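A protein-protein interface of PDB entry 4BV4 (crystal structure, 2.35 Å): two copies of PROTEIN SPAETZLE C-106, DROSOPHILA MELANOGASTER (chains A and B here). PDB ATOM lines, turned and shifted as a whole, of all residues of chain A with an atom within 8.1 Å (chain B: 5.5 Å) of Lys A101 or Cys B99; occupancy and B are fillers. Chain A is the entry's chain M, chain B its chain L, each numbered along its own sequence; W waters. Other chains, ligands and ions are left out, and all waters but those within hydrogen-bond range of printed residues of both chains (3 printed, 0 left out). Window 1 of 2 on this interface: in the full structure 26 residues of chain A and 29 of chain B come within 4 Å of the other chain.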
ATOM      1  N   LEU A  10      -6.649  27.286  -1.715  1.00  0.00           N
ATOM      2  CA  LEU A  10      -6.114  27.279  -0.361  1.00  0.00           C
ATOM      3  C   LEU A  10      -5.803  25.855   0.077  1.00  0.00           C
ATOM      4  O   LEU A  10      -4.889  25.642   0.878  1.00  0.00           O
ATOM      5  CB  LEU A  10      -7.110  27.944   0.610  1.00  0.00           C
ATOM      6  CG  LEU A  10      -7.070  29.468   0.667  1.00  0.00           C
ATOM      7  CD1 LEU A  10      -8.162  30.077  -0.170  1.00  0.00           C
ATOM      8  CD2 LEU A  10      -7.214  29.955   2.085  1.00  0.00           C
ATOM      9  N   CYS A  11      -6.573  24.886  -0.443  1.00  0.00           N
ATOM     10  CA  CYS A  11      -6.384  23.458  -0.168  1.00  0.00           C
ATOM     11  C   CYS A  11      -6.417  22.681  -1.481  1.00  0.00           C
ATOM     12  O   CYS A  11      -7.296  22.923  -2.314  1.00  0.00           O
ATOM     13  CB  CYS A  11      -7.443  22.932   0.792  1.00  0.00           C
ATOM     14  SG  CYS A  11      -7.469  23.746   2.405  1.00  0.00           S
ATOM     15  N   ARG A  12      -5.494  21.736  -1.650  1.00  0.00           N
ATOM     16  CA  ARG A  12      -5.408  20.860  -2.822  1.00  0.00           C
ATOM     17  C   ARG A  12      -5.971  19.490  -2.504  1.00  0.00           C
ATOM     18  O   ARG A  12      -5.627  18.883  -1.477  1.00  0.00           O
ATOM     19  CB  ARG A  12      -3.952  20.694  -3.326  1.00  0.00           C
ATOM     20  CG  ARG A  12      -3.287  21.953  -3.859  1.00  0.00           C
ATOM     21  CD  ARG A  12      -3.916  22.484  -5.136  1.00  0.00           C
ATOM     22  NE  ARG A  12      -3.527  23.881  -5.349  1.00  0.00           N
ATOM     23  CZ  ARG A  12      -3.756  24.579  -6.457  1.00  0.00           C
ATOM     24  NH1 ARG A  12      -4.390  24.023  -7.485  1.00  0.00           N
ATOM     25  NH2 ARG A  12      -3.337  25.830  -6.552  1.00  0.00           N
ATOM     26  N   SER A  13      -6.799  18.986  -3.418  1.00  0.00           N
ATOM     27  CA  SER A  13      -7.379  17.654  -3.315  1.00  0.00           C
ATOM     28  C   SER A  13      -6.801  16.723  -4.388  1.00  0.00           C
ATOM     29  O   SER A  13      -6.234  17.189  -5.384  1.00  0.00           O
ATOM     30  CB  SER A  13      -8.899  17.724  -3.423  1.00  0.00           C
ATOM     31  OG  SER A  13      -9.291  18.374  -4.619  1.00  0.00           O
ATOM     32  N   GLU A  46     -13.094  13.306  -3.975  1.00  0.00           N
ATOM     33  CA  GLU A  46     -12.040  14.312  -3.858  1.00  0.00           C
ATOM     34  C   GLU A  46     -11.556  14.320  -2.422  1.00  0.00           C
ATOM     35  O   GLU A  46     -12.330  14.624  -1.514  1.00  0.00           O
ATOM     36  CB  GLU A  46     -12.495  15.698  -4.321  1.00  0.00           C
ATOM     37  CG  GLU A  46     -12.761  15.778  -5.815  1.00  0.00           C
ATOM     38  CD  GLU A  46     -11.564  15.862  -6.750  1.00  0.00           C
ATOM     39  OE1 GLU A  46     -10.437  16.135  -6.273  1.00  0.00           O
ATOM     40  OE2 GLU A  46     -11.776  15.727  -7.979  1.00  0.00           O
ATOM     41  N   GLU A  47     -10.304  13.888  -2.214  1.00  0.00           N
ATOM     42  CA  GLU A  47      -9.717  13.799  -0.880  1.00  0.00           C
ATOM     43  C   GLU A  47      -8.588  14.800  -0.677  1.00  0.00           C
ATOM     44  O   GLU A  47      -7.863  15.096  -1.627  1.00  0.00           O
ATOM     45  CB  GLU A  47      -9.200  12.377  -0.603  1.00  0.00           C
ATOM     46  CG  GLU A  47     -10.320  11.369  -0.439  1.00  0.00           C
ATOM     47  CD  GLU A  47     -10.097  10.327   0.638  1.00  0.00           C
ATOM     48  OE1 GLU A  47      -9.419   9.311   0.351  1.00  0.00           O
ATOM     49  OE2 GLU A  47     -10.634  10.508   1.758  1.00  0.00           O
ATOM     50  N   CYS A  48      -8.428  15.297   0.573  1.00  0.00           N
ATOM     51  CA  CYS A  48      -7.335  16.186   0.976  1.00  0.00           C
ATOM     52  C   CYS A  48      -6.003  15.478   0.775  1.00  0.00           C
ATOM     53  O   CYS A  48      -5.869  14.322   1.170  1.00  0.00           O
ATOM     54  CB  CYS A  48      -7.499  16.622   2.433  1.00  0.00           C
ATOM     55  SG  CYS A  48      -8.943  17.657   2.749  1.00  0.00           S
ATOM     56  N   ASP A  52      -4.401  16.867   8.949  1.00  0.00           N
ATOM     57  CA  ASP A  52      -5.054  18.172   8.732  1.00  0.00           C
ATOM     58  C   ASP A  52      -3.989  19.284   8.649  1.00  0.00           C
ATOM     59  O   ASP A  52      -3.477  19.765   9.661  1.00  0.00           O
ATOM     60  CB  ASP A  52      -6.081  18.456   9.842  1.00  0.00           C
ATOM     61  CG  ASP A  52      -7.246  17.484   9.861  1.00  0.00           C
ATOM     62  OD1 ASP A  52      -8.138  17.606   8.986  1.00  0.00           O
ATOM     63  OD2 ASP A  52      -7.282  16.615  10.766  1.00  0.00           O
ATOM     64  N   GLN A  53      -3.650  19.653   7.412  1.00  0.00           N
ATOM     65  CA  GLN A  53      -2.611  20.612   7.043  1.00  0.00           C
ATOM     66  C   GLN A  53      -3.107  22.051   7.067  1.00  0.00           C
ATOM     67  O   GLN A  53      -4.282  22.284   6.763  1.00  0.00           O
ATOM     68  CB  GLN A  53      -2.110  20.308   5.604  1.00  0.00           C
ATOM     69  CG  GLN A  53      -1.967  18.834   5.218  1.00  0.00           C
ATOM     70  CD  GLN A  53      -0.861  18.125   5.962  1.00  0.00           C
ATOM     71  OE1 GLN A  53       0.322  18.488   5.879  1.00  0.00           O
ATOM     72  NE2 GLN A  53      -1.229  17.073   6.683  1.00  0.00           N
ATOM     73  N   CYS A  55      -3.913  25.732   5.515  1.00  0.00           N
ATOM     74  CA  CYS A  55      -4.245  26.218   4.181  1.00  0.00           C
ATOM     75  C   CYS A  55      -3.070  27.021   3.628  1.00  0.00           C
ATOM     76  O   CYS A  55      -2.281  27.581   4.395  1.00  0.00           O
ATOM     77  CB  CYS A  55      -5.501  27.081   4.211  1.00  0.00           C
ATOM     78  SG  CYS A  55      -6.905  26.359   5.089  1.00  0.00           S
ATOM     79  N   PRO A  67      -6.251  28.638   9.940  1.00  0.00           N
ATOM     80  CA  PRO A  67      -6.746  28.079   8.671  1.00  0.00           C
ATOM     81  C   PRO A  67      -6.210  26.670   8.467  1.00  0.00           C
ATOM     82  O   PRO A  67      -5.006  26.454   8.317  1.00  0.00           O
ATOM     83  CB  PRO A  67      -6.252  29.063   7.598  1.00  0.00           C
ATOM     84  CG  PRO A  67      -5.631  30.184   8.328  1.00  0.00           C
ATOM     85  CD  PRO A  67      -5.283  29.722   9.702  1.00  0.00           C
ATOM     86  N   ILE A  68      -7.128  25.698   8.498  1.00  0.00           N
ATOM     87  CA  ILE A  68      -6.812  24.282   8.361  1.00  0.00           C
ATOM     88  C   ILE A  68      -7.664  23.681   7.256  1.00  0.00           C
ATOM     89  O   ILE A  68      -8.857  23.967   7.174  1.00  0.00           O
ATOM     90  CB  ILE A  68      -7.013  23.555   9.733  1.00  0.00           C
ATOM     91  CG1 ILE A  68      -5.945  23.959  10.784  1.00  0.00           C
ATOM     92  CG2 ILE A  68      -7.136  22.025   9.603  1.00  0.00           C
ATOM     93  CD1 ILE A  68      -4.445  23.744  10.489  1.00  0.00           C
ATOM     94  N   CYS A  69      -7.036  22.862   6.402  1.00  0.00           N
ATOM     95  CA  CYS A  69      -7.679  22.122   5.312  1.00  0.00           C
ATOM     96  C   CYS A  69      -8.512  21.005   5.895  1.00  0.00           C
ATOM     97  O   CYS A  69      -8.011  20.166   6.642  1.00  0.00           O
ATOM     98  CB  CYS A  69      -6.636  21.595   4.333  1.00  0.00           C
ATOM     99  SG  CYS A  69      -5.871  22.884   3.325  1.00  0.00           S
ATOM    100  N   LYS A  70      -9.791  21.028   5.594  1.00  0.00           N
ATOM    101  CA  LYS A  70     -10.744  20.078   6.138  1.00  0.00           C
ATOM    102  C   LYS A  70     -11.472  19.310   5.047  1.00  0.00           C
ATOM    103  O   LYS A  70     -11.926  19.897   4.059  1.00  0.00           O
ATOM    104  CB  LYS A  70     -11.749  20.827   7.029  1.00  0.00           C
ATOM    105  CG  LYS A  70     -11.866  20.273   8.444  1.00  0.00           C
ATOM    106  CD  LYS A  70     -10.652  20.580   9.327  1.00  0.00           C
ATOM    107  CE  LYS A  70     -10.578  19.619  10.489  1.00  0.00           C
ATOM    108  NZ  LYS A  70      -9.282  19.718  11.207  1.00  0.00           N
ATOM    109  N   GLN A  71     -11.587  17.986   5.250  1.00  0.00           N
ATOM    110  CA  GLN A  71     -12.301  17.083   4.366  1.00  0.00           C
ATOM    111  C   GLN A  71     -13.841  17.260   4.498  1.00  0.00           C
ATOM    112  O   GLN A  71     -14.409  17.150   5.594  1.00  0.00           O
ATOM    113  CB  GLN A  71     -11.895  15.633   4.650  1.00  0.00           C
ATOM    114  CG  GLN A  71     -12.547  14.595   3.729  1.00  0.00           C
ATOM    115  CD  GLN A  71     -12.016  14.672   2.324  1.00  0.00           C
ATOM    116  OE1 GLN A  71     -10.840  14.380   2.065  1.00  0.00           O
ATOM    117  NE2 GLN A  71     -12.865  15.094   1.400  1.00  0.00           N
ATOM    118  N   HIS A  72     -14.482  17.530   3.341  1.00  0.00           N
ATOM    119  CA  HIS A  72     -15.914  17.685   3.124  1.00  0.00           C
ATOM    120  C   HIS A  72     -16.489  16.347   2.643  1.00  0.00           C
ATOM    121  O   HIS A  72     -15.782  15.537   2.023  1.00  0.00           O
ATOM    122  CB  HIS A  72     -16.161  18.804   2.083  1.00  0.00           C
ATOM    123  CG  HIS A  72     -17.600  19.101   1.768  1.00  0.00           C
ATOM    124  ND1 HIS A  72     -18.216  18.590   0.633  1.00  0.00           N
ATOM    125  CD2 HIS A  72     -18.496  19.857   2.443  1.00  0.00           C
ATOM    126  CE1 HIS A  72     -19.460  19.031   0.669  1.00  0.00           C
ATOM    127  NE2 HIS A  72     -19.671  19.813   1.730  1.00  0.00           N
ATOM    128  N   TYR A  73     -17.769  16.115   2.948  1.00  0.00           N
ATOM    129  CA  TYR A  73     -18.485  14.901   2.568  1.00  0.00           C
ATOM    130  C   TYR A  73     -19.871  15.206   2.026  1.00  0.00           C
ATOM    131  O   TYR A  73     -20.514  16.157   2.475  1.00  0.00           O
ATOM    132  CB  TYR A  73     -18.621  13.951   3.768  1.00  0.00           C
ATOM    133  CG  TYR A  73     -17.302  13.443   4.303  1.00  0.00           C
ATOM    134  CD1 TYR A  73     -16.695  12.315   3.756  1.00  0.00           C
ATOM    135  CD2 TYR A  73     -16.685  14.056   5.389  1.00  0.00           C
ATOM    136  CE1 TYR A  73     -15.482  11.836   4.250  1.00  0.00           C
ATOM    137  CE2 TYR A  73     -15.478  13.578   5.901  1.00  0.00           C
ATOM    138  CZ  TYR A  73     -14.884  12.463   5.332  1.00  0.00           C
ATOM    139  OH  TYR A  73     -13.699  11.986   5.831  1.00  0.00           O
ATOM    140  N   THR A  74     -20.333  14.381   1.076  1.00  0.00           N
ATOM    141  CA  THR A  74     -21.681  14.445   0.525  1.00  0.00           C
ATOM    142  C   THR A  74     -22.371  13.155   0.966  1.00  0.00           C
ATOM    143  O   THR A  74     -21.736  12.097   0.950  1.00  0.00           O
ATOM    144  CB  THR A  74     -21.685  14.684  -1.000  1.00  0.00           C
ATOM    145  OG1 THR A  74     -20.846  13.739  -1.652  1.00  0.00           O
ATOM    146  CG2 THR A  74     -21.267  16.098  -1.379  1.00  0.00           C
ATOM    147  N   SER A  98     -15.925  14.529  -0.931  1.00  0.00           N
ATOM    148  CA  SER A  98     -16.184  15.285  -2.163  1.00  0.00           C
ATOM    149  C   SER A  98     -15.408  16.600  -2.297  1.00  0.00           C
ATOM    150  O   SER A  98     -15.417  17.193  -3.382  1.00  0.00           O
ATOM    151  CB  SER A  98     -17.672  15.597  -2.258  1.00  0.00           C
ATOM    152  OG  SER A  98     -18.034  16.494  -1.220  1.00  0.00           O
ATOM    153  N   CYS A  99     -14.780  17.075  -1.209  1.00  0.00           N
ATOM    154  CA  CYS A  99     -14.046  18.333  -1.215  1.00  0.00           C
ATOM    155  C   CYS A  99     -13.080  18.418  -0.077  1.00  0.00           C
ATOM    156  O   CYS A  99     -13.274  17.841   0.991  1.00  0.00           O
ATOM    157  CB  CYS A  99     -15.009  19.517  -1.155  1.00  0.00           C
ATOM    158  SG  CYS A  99     -15.168  20.431  -2.708  1.00  0.00           S
ATOM    159  N   CYS A 100     -12.064  19.227  -0.301  1.00  0.00           N
ATOM    160  CA  CYS A 100     -11.133  19.675   0.692  1.00  0.00           C
ATOM    161  C   CYS A 100     -11.318  21.173   0.771  1.00  0.00           C
ATOM    162  O   CYS A 100     -11.179  21.844  -0.243  1.00  0.00           O
ATOM    163  CB  CYS A 100      -9.703  19.287   0.352  1.00  0.00           C
ATOM    164  SG  CYS A 100      -8.577  19.416   1.756  1.00  0.00           S
ATOM    165  N   LYS A 101     -11.705  21.694   1.938  1.00  0.00           N
ATOM    166  CA  LYS A 101     -11.986  23.121   2.096  1.00  0.00           C
ATOM    167  C   LYS A 101     -11.173  23.736   3.205  1.00  0.00           C
ATOM    168  O   LYS A 101     -10.803  23.036   4.142  1.00  0.00           O
ATOM    169  CB  LYS A 101     -13.480  23.362   2.397  1.00  0.00           C
ATOM    170  CG  LYS A 101     -14.402  23.263   1.214  1.00  0.00           C
ATOM    171  CD  LYS A 101     -15.677  24.134   1.378  1.00  0.00           C
ATOM    172  CE  LYS A 101     -16.560  23.906   2.595  1.00  0.00           C
ATOM    173  NZ  LYS A 101     -16.778  22.464   2.894  1.00  0.00           N
ATOM    174  N   CYS A 102     -10.979  25.066   3.148  1.00  0.00           N
ATOM    175  CA  CYS A 102     -10.235  25.766   4.185  1.00  0.00           C
ATOM    176  C   CYS A 102     -11.162  26.182   5.311  1.00  0.00           C
ATOM    177  O   CYS A 102     -12.055  26.997   5.096  1.00  0.00           O
ATOM    178  CB  CYS A 102      -9.473  26.965   3.627  1.00  0.00           C
ATOM    179  SG  CYS A 102      -8.380  27.753   4.844  1.00  0.00           S
ATOM    180  N   ALA A 103     -10.943  25.634   6.515  1.00  0.00           N
ATOM    181  CA  ALA A 103     -11.751  25.990   7.677  1.00  0.00           C
ATOM    182  C   ALA A 103     -10.978  26.952   8.558  1.00  0.00           C
ATOM    183  O   ALA A 103      -9.867  26.639   8.977  1.00  0.00           O
ATOM    184  CB  ALA A 103     -12.145  24.746   8.453  1.00  0.00           C
ATOM    185  N   LEU A 104     -11.504  28.165   8.743  1.00  0.00           N
ATOM    186  CA  LEU A 104     -10.903  29.150   9.638  1.00  0.00           C
ATOM    187  C   LEU A 104     -11.425  28.783  11.007  1.00  0.00           C
ATOM    188  O   LEU A 104     -12.585  29.070  11.325  1.00  0.00           O
ATOM    189  CB  LEU A 104     -11.242  30.604   9.247  1.00  0.00           C
ATOM    190  CG  LEU A 104     -11.026  31.064   7.806  1.00  0.00           C
ATOM    191  CD1 LEU A 104     -11.792  32.364   7.546  1.00  0.00           C
ATOM    192  CD2 LEU A 104      -9.560  31.270   7.499  1.00  0.00           C
ATOM    193  N   PHE B   9     -16.037  29.408   7.084  1.00  0.00           N
ATOM    194  CA  PHE B   9     -15.528  29.220   5.731  1.00  0.00           C
ATOM    195  C   PHE B   9     -15.575  30.554   4.983  1.00  0.00           C
ATOM    196  O   PHE B   9     -16.331  31.459   5.359  1.00  0.00           O
ATOM    197  CB  PHE B   9     -16.324  28.120   4.996  1.00  0.00           C
ATOM    198  CG  PHE B   9     -16.174  26.750   5.621  1.00  0.00           C
ATOM    199  CD1 PHE B   9     -15.118  25.917   5.267  1.00  0.00           C
ATOM    200  CD2 PHE B   9     -17.077  26.301   6.579  1.00  0.00           C
ATOM    201  CE1 PHE B   9     -14.969  24.656   5.858  1.00  0.00           C
ATOM    202  CE2 PHE B   9     -16.921  25.045   7.176  1.00  0.00           C
ATOM    203  CZ  PHE B   9     -15.868  24.231   6.811  1.00  0.00           C
ATOM    204  N   GLU B  46     -23.611  20.618  -0.921  1.00  0.00           N
ATOM    205  CA  GLU B  46     -23.282  21.968  -0.497  1.00  0.00           C
ATOM    206  C   GLU B  46     -23.275  22.874  -1.726  1.00  0.00           C
ATOM    207  O   GLU B  46     -22.535  22.634  -2.680  1.00  0.00           O
ATOM    208  CB  GLU B  46     -21.951  22.003   0.248  1.00  0.00           C
ATOM    209  CG  GLU B  46     -21.599  23.384   0.749  1.00  0.00           C
ATOM    210  CD  GLU B  46     -20.149  23.569   1.152  1.00  0.00           C
ATOM    211  OE1 GLU B  46     -19.680  22.814   2.035  1.00  0.00           O
ATOM    212  OE2 GLU B  46     -19.497  24.495   0.615  1.00  0.00           O
ATOM    213  N   CYS B  48     -23.316  27.015  -3.282  1.00  0.00           N
ATOM    214  CA  CYS B  48     -22.927  28.397  -3.005  1.00  0.00           C
ATOM    215  C   CYS B  48     -24.151  29.245  -2.760  1.00  0.00           C
ATOM    216  O   CYS B  48     -25.123  29.168  -3.519  1.00  0.00           O
ATOM    217  CB  CYS B  48     -22.119  28.990  -4.152  1.00  0.00           C
ATOM    218  SG  CYS B  48     -20.537  28.187  -4.469  1.00  0.00           S
ATOM    219  N   LYS B  70     -16.554  29.620  -5.886  1.00  0.00           N
ATOM    220  CA  LYS B  70     -16.811  28.757  -7.023  1.00  0.00           C
ATOM    221  C   LYS B  70     -17.486  27.464  -6.597  1.00  0.00           C
ATOM    222  O   LYS B  70     -17.063  26.810  -5.642  1.00  0.00           O
ATOM    223  CB  LYS B  70     -15.469  28.460  -7.723  1.00  0.00           C
ATOM    224  CG  LYS B  70     -15.465  28.784  -9.206  1.00  0.00           C
ATOM    225  CD  LYS B  70     -15.406  30.265  -9.511  1.00  0.00           C
ATOM    226  CE  LYS B  70     -15.855  30.536 -10.924  1.00  0.00           C
ATOM    227  NZ  LYS B  70     -16.090  31.985 -11.160  1.00  0.00           N
ATOM    228  N   GLN B  71     -18.542  27.104  -7.315  1.00  0.00           N
ATOM    229  CA  GLN B  71     -19.277  25.855  -7.140  1.00  0.00           C
ATOM    230  C   GLN B  71     -18.482  24.708  -7.790  1.00  0.00           C
ATOM    231  O   GLN B  71     -18.176  24.767  -8.985  1.00  0.00           O
ATOM    232  CB  GLN B  71     -20.684  25.964  -7.766  1.00  0.00           C
ATOM    233  CG  GLN B  71     -21.546  24.705  -7.599  1.00  0.00           C
ATOM    234  CD  GLN B  71     -21.975  24.500  -6.177  1.00  0.00           C
ATOM    235  OE1 GLN B  71     -22.761  25.263  -5.645  1.00  0.00           O
ATOM    236  NE2 GLN B  71     -21.447  23.489  -5.525  1.00  0.00           N
ATOM    237  N   HIS B  72     -18.141  23.686  -7.015  1.00  0.00           N
ATOM    238  CA  HIS B  72     -17.426  22.542  -7.553  1.00  0.00           C
ATOM    239  C   HIS B  72     -18.399  21.396  -7.758  1.00  0.00           C
ATOM    240  O   HIS B  72     -19.512  21.419  -7.227  1.00  0.00           O
ATOM    241  CB  HIS B  72     -16.240  22.168  -6.665  1.00  0.00           C
ATOM    242  CG  HIS B  72     -15.059  23.072  -6.869  1.00  0.00           C
ATOM    243  ND1 HIS B  72     -13.829  22.571  -7.211  1.00  0.00           N
ATOM    244  CD2 HIS B  72     -14.979  24.420  -6.825  1.00  0.00           C
ATOM    245  CE1 HIS B  72     -13.032  23.620  -7.335  1.00  0.00           C
ATOM    246  NE2 HIS B  72     -13.687  24.752  -7.130  1.00  0.00           N
ATOM    247  N   TYR B  73     -18.043  20.460  -8.632  1.00  0.00           N
ATOM    248  CA  TYR B  73     -18.919  19.341  -8.961  1.00  0.00           C
ATOM    249  C   TYR B  73     -18.152  18.056  -8.943  1.00  0.00           C
ATOM    250  O   TYR B  73     -16.932  18.057  -9.088  1.00  0.00           O
ATOM    251  CB  TYR B  73     -19.595  19.532 -10.339  1.00  0.00           C
ATOM    252  CG  TYR B  73     -20.404  20.803 -10.466  1.00  0.00           C
ATOM    253  CD1 TYR B  73     -19.796  22.011 -10.802  1.00  0.00           C
ATOM    254  CD2 TYR B  73     -21.786  20.797 -10.281  1.00  0.00           C
ATOM    255  CE1 TYR B  73     -20.538  23.177 -10.948  1.00  0.00           C
ATOM    256  CE2 TYR B  73     -22.533  21.967 -10.389  1.00  0.00           C
ATOM    257  CZ  TYR B  73     -21.907  23.148 -10.751  1.00  0.00           C
ATOM    258  OH  TYR B  73     -22.616  24.314 -10.856  1.00  0.00           O
ATOM    259  N   PRO B  97     -23.292  18.859  -7.769  1.00  0.00           N
ATOM    260  CA  PRO B  97     -22.506  19.825  -6.989  1.00  0.00           C
ATOM    261  C   PRO B  97     -21.894  19.179  -5.749  1.00  0.00           C
ATOM    262  O   PRO B  97     -22.436  18.207  -5.251  1.00  0.00           O
ATOM    263  CB  PRO B  97     -23.532  20.913  -6.627  1.00  0.00           C
ATOM    264  CG  PRO B  97     -24.846  20.269  -6.758  1.00  0.00           C
ATOM    265  CD  PRO B  97     -24.708  19.274  -7.854  1.00  0.00           C
ATOM    266  N   SER B  98     -20.718  19.641  -5.322  1.00  0.00           N
ATOM    267  CA  SER B  98     -20.058  19.069  -4.157  1.00  0.00           C
ATOM    268  C   SER B  98     -19.944  20.102  -3.045  1.00  0.00           C
ATOM    269  O   SER B  98     -20.570  19.955  -1.993  1.00  0.00           O
ATOM    270  CB  SER B  98     -18.687  18.519  -4.530  1.00  0.00           C
ATOM    271  OG  SER B  98     -17.926  19.471  -5.249  1.00  0.00           O
ATOM    272  N   CYS B  99     -19.181  21.165  -3.292  1.00  0.00           N
ATOM    273  CA  CYS B  99     -18.914  22.186  -2.304  1.00  0.00           C
ATOM    274  C   CYS B  99     -18.661  23.530  -2.978  1.00  0.00           C
ATOM    275  O   CYS B  99     -18.425  23.603  -4.189  1.00  0.00           O
ATOM    276  CB  CYS B  99     -17.713  21.763  -1.460  1.00  0.00           C
ATOM    277  SG  CYS B  99     -16.109  22.163  -2.210  1.00  0.00           S
ATOM    278  N   CYS B 100     -18.669  24.587  -2.161  1.00  0.00           N
ATOM    279  CA  CYS B 100     -18.372  25.948  -2.566  1.00  0.00           C
ATOM    280  C   CYS B 100     -16.979  26.215  -2.089  1.00  0.00           C
ATOM    281  O   CYS B 100     -16.725  26.116  -0.889  1.00  0.00           O
ATOM    282  CB  CYS B 100     -19.377  26.934  -1.980  1.00  0.00           C
ATOM    283  SG  CYS B 100     -19.378  28.533  -2.822  1.00  0.00           S
ATOM    284  N   LYS B 101     -16.052  26.436  -3.010  1.00  0.00           N
ATOM    285  CA  LYS B 101     -14.643  26.662  -2.673  1.00  0.00           C
ATOM    286  C   LYS B 101     -14.217  28.053  -3.098  1.00  0.00           C
ATOM    287  O   LYS B 101     -14.716  28.558  -4.107  1.00  0.00           O
ATOM    288  CB  LYS B 101     -13.766  25.618  -3.386  1.00  0.00           C
ATOM    289  CG  LYS B 101     -12.984  24.664  -2.505  1.00  0.00           C
ATOM    290  CD  LYS B 101     -12.106  23.800  -3.416  1.00  0.00           C
ATOM    291  CE  LYS B 101     -10.820  23.286  -2.811  1.00  0.00           C
ATOM    292  NZ  LYS B 101      -9.863  24.364  -2.456  1.00  0.00           N
HETATM  293  O   HOH W   1      -9.415  27.102  -2.233  1.00  0.00           O
HETATM  294  O   HOH W   2     -10.287  25.802  -0.031  1.00  0.00           O
HETATM  295  O   HOH W   3     -15.223  18.476  -5.857  1.00  0.00           O
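The side-chain carboxylate (OE1) of Glu B46 sits at hydrogen-bond distance from a ring nitrogen (NE2) of His A72.
The side-chain carboxylate (OE1) of Glu B46 lies within salt-bridge range of the side-chain amino group (NZ) of Lys A101 (3.0 Å).
The side-chain sulfur (SG) of Cys B99 is disulfide-bonded to the side-chain sulfur (SG) of Cys A99 (2.0 Å).
The side-chain amino group (NZ) of Lys B101 is in hydrogen-bond range of the backbone carbonyl oxygen (O) of Cys A11 (2.9 Å).
SG of Cys A69 is disulfide-bonded to SG of Cys A11, at 2.0 Å.
The side-chain sulfur (SG) of Cys A55 forms a disulfide with the side-chain sulfur (SG) of Cys A102 (2.0 Å).
OE2 of Glu B46 is in hydrogen-bond range of N of Cys B100, 2.9 Å away.
SG of Cys A48 forms a disulfide with SG of Cys A100 (2.1 Å).
SG of Cys B100 forms a disulfide with SG of Cys B48 (2.0 Å).
O of Cys A99 sits at hydrogen-bond distance from NE2 of Gln A71 (2.8 Å).
Among the printed residues, merely in contact across the chains: His A72 with Ser B98 (3.0 Å), His A72 with Cys B99 (3.8 Å), Thr A74 with Ser B98 (3.97 Å), Ser A98 with Ser B98 (3.7 Å), Cys A99 with Ser B98 (3.9 Å), Cys A100 with Lys B101 (3.0 Å), Lys A101 with Phe B9 (3.6 Å), Lys A101 with Cys B99 (3.98 Å), Lys A101 with Cys B100 (3.2 Å), Cys A102 with Phe B9 (3.3 Å) and Ala A103 with Phe B9 (3.8 Å).
Of the printed residues of chain B, Lys A101 touches Phe B9, Glu B46, Cys B99 and Cys B100.
Of the printed residues of chain A, Phe B9 touches Lys A101, Cys A102 and Ala A103.
Gln B71 touches none of the printed residues of chain A.
Of chain A, only His A72, Thr A74, Ser A98 and Cys A99 come within 4 Å of Ser B98.
Of the printed residues of chain A, Cys B99 touches His A72, Cys A99 and Lys A101.
Of the printed residues of chain A, Cys B100 touches Lys A101 (3.2 Å).
The nearest printed residue of chain B that does not touch Lys A101 is Lys B101 (4.2 Å).
Of the 12 printed residues of chain B, 6 touch a printed residue of chain A.
Hydrophobic or aromatic side chains of chain B that line the printed part of chain A: Phe B9.
Of the 25 printed residues of chain A, 9 touch a printed residue of chain B.
Hydrophobic or aromatic side chains of chain A within 4 Å of the printed part of chain B: His A72 and Ala A103.
Among the printed residues, 15 pairs touch across the chains.
Among the printed residues, Asp or Glu carboxylates within 4 Å of a Lys or Arg side-chain nitrogen of the other chain: Lys A101 with Glu B46 (3.0 Å).
His A72 touches Glu B46, but with the chains exchanged Glu A46 does not touch His B72 (7.0 Å).
Cys A99 touches Ser B98, but with the chains exchanged Ser A98 does not touch Cys B99 (5.2 Å).
Lys A101 touches Glu B46, but with the chains exchanged Glu A46 does not touch Lys B101 (7.9 Å).
Lys A101 touches Cys B99, but with the chains exchanged Cys A99 does not touch Lys B101 (4.6 Å).
10 positions are printed for both chains.
Water W1 bridges NZ of Lys B101 and N of Leu A10.
Water W3 lies within hydrogen-bond range of O of Ser A98 (2.8 Å), OG of Ser B98 (2.9 Å) and SG of Cys A99 (3.7 Å).
Water W2 bridges NZ of Lys B101 (2.9 Å) and N of Cys A102 (3.3 Å).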
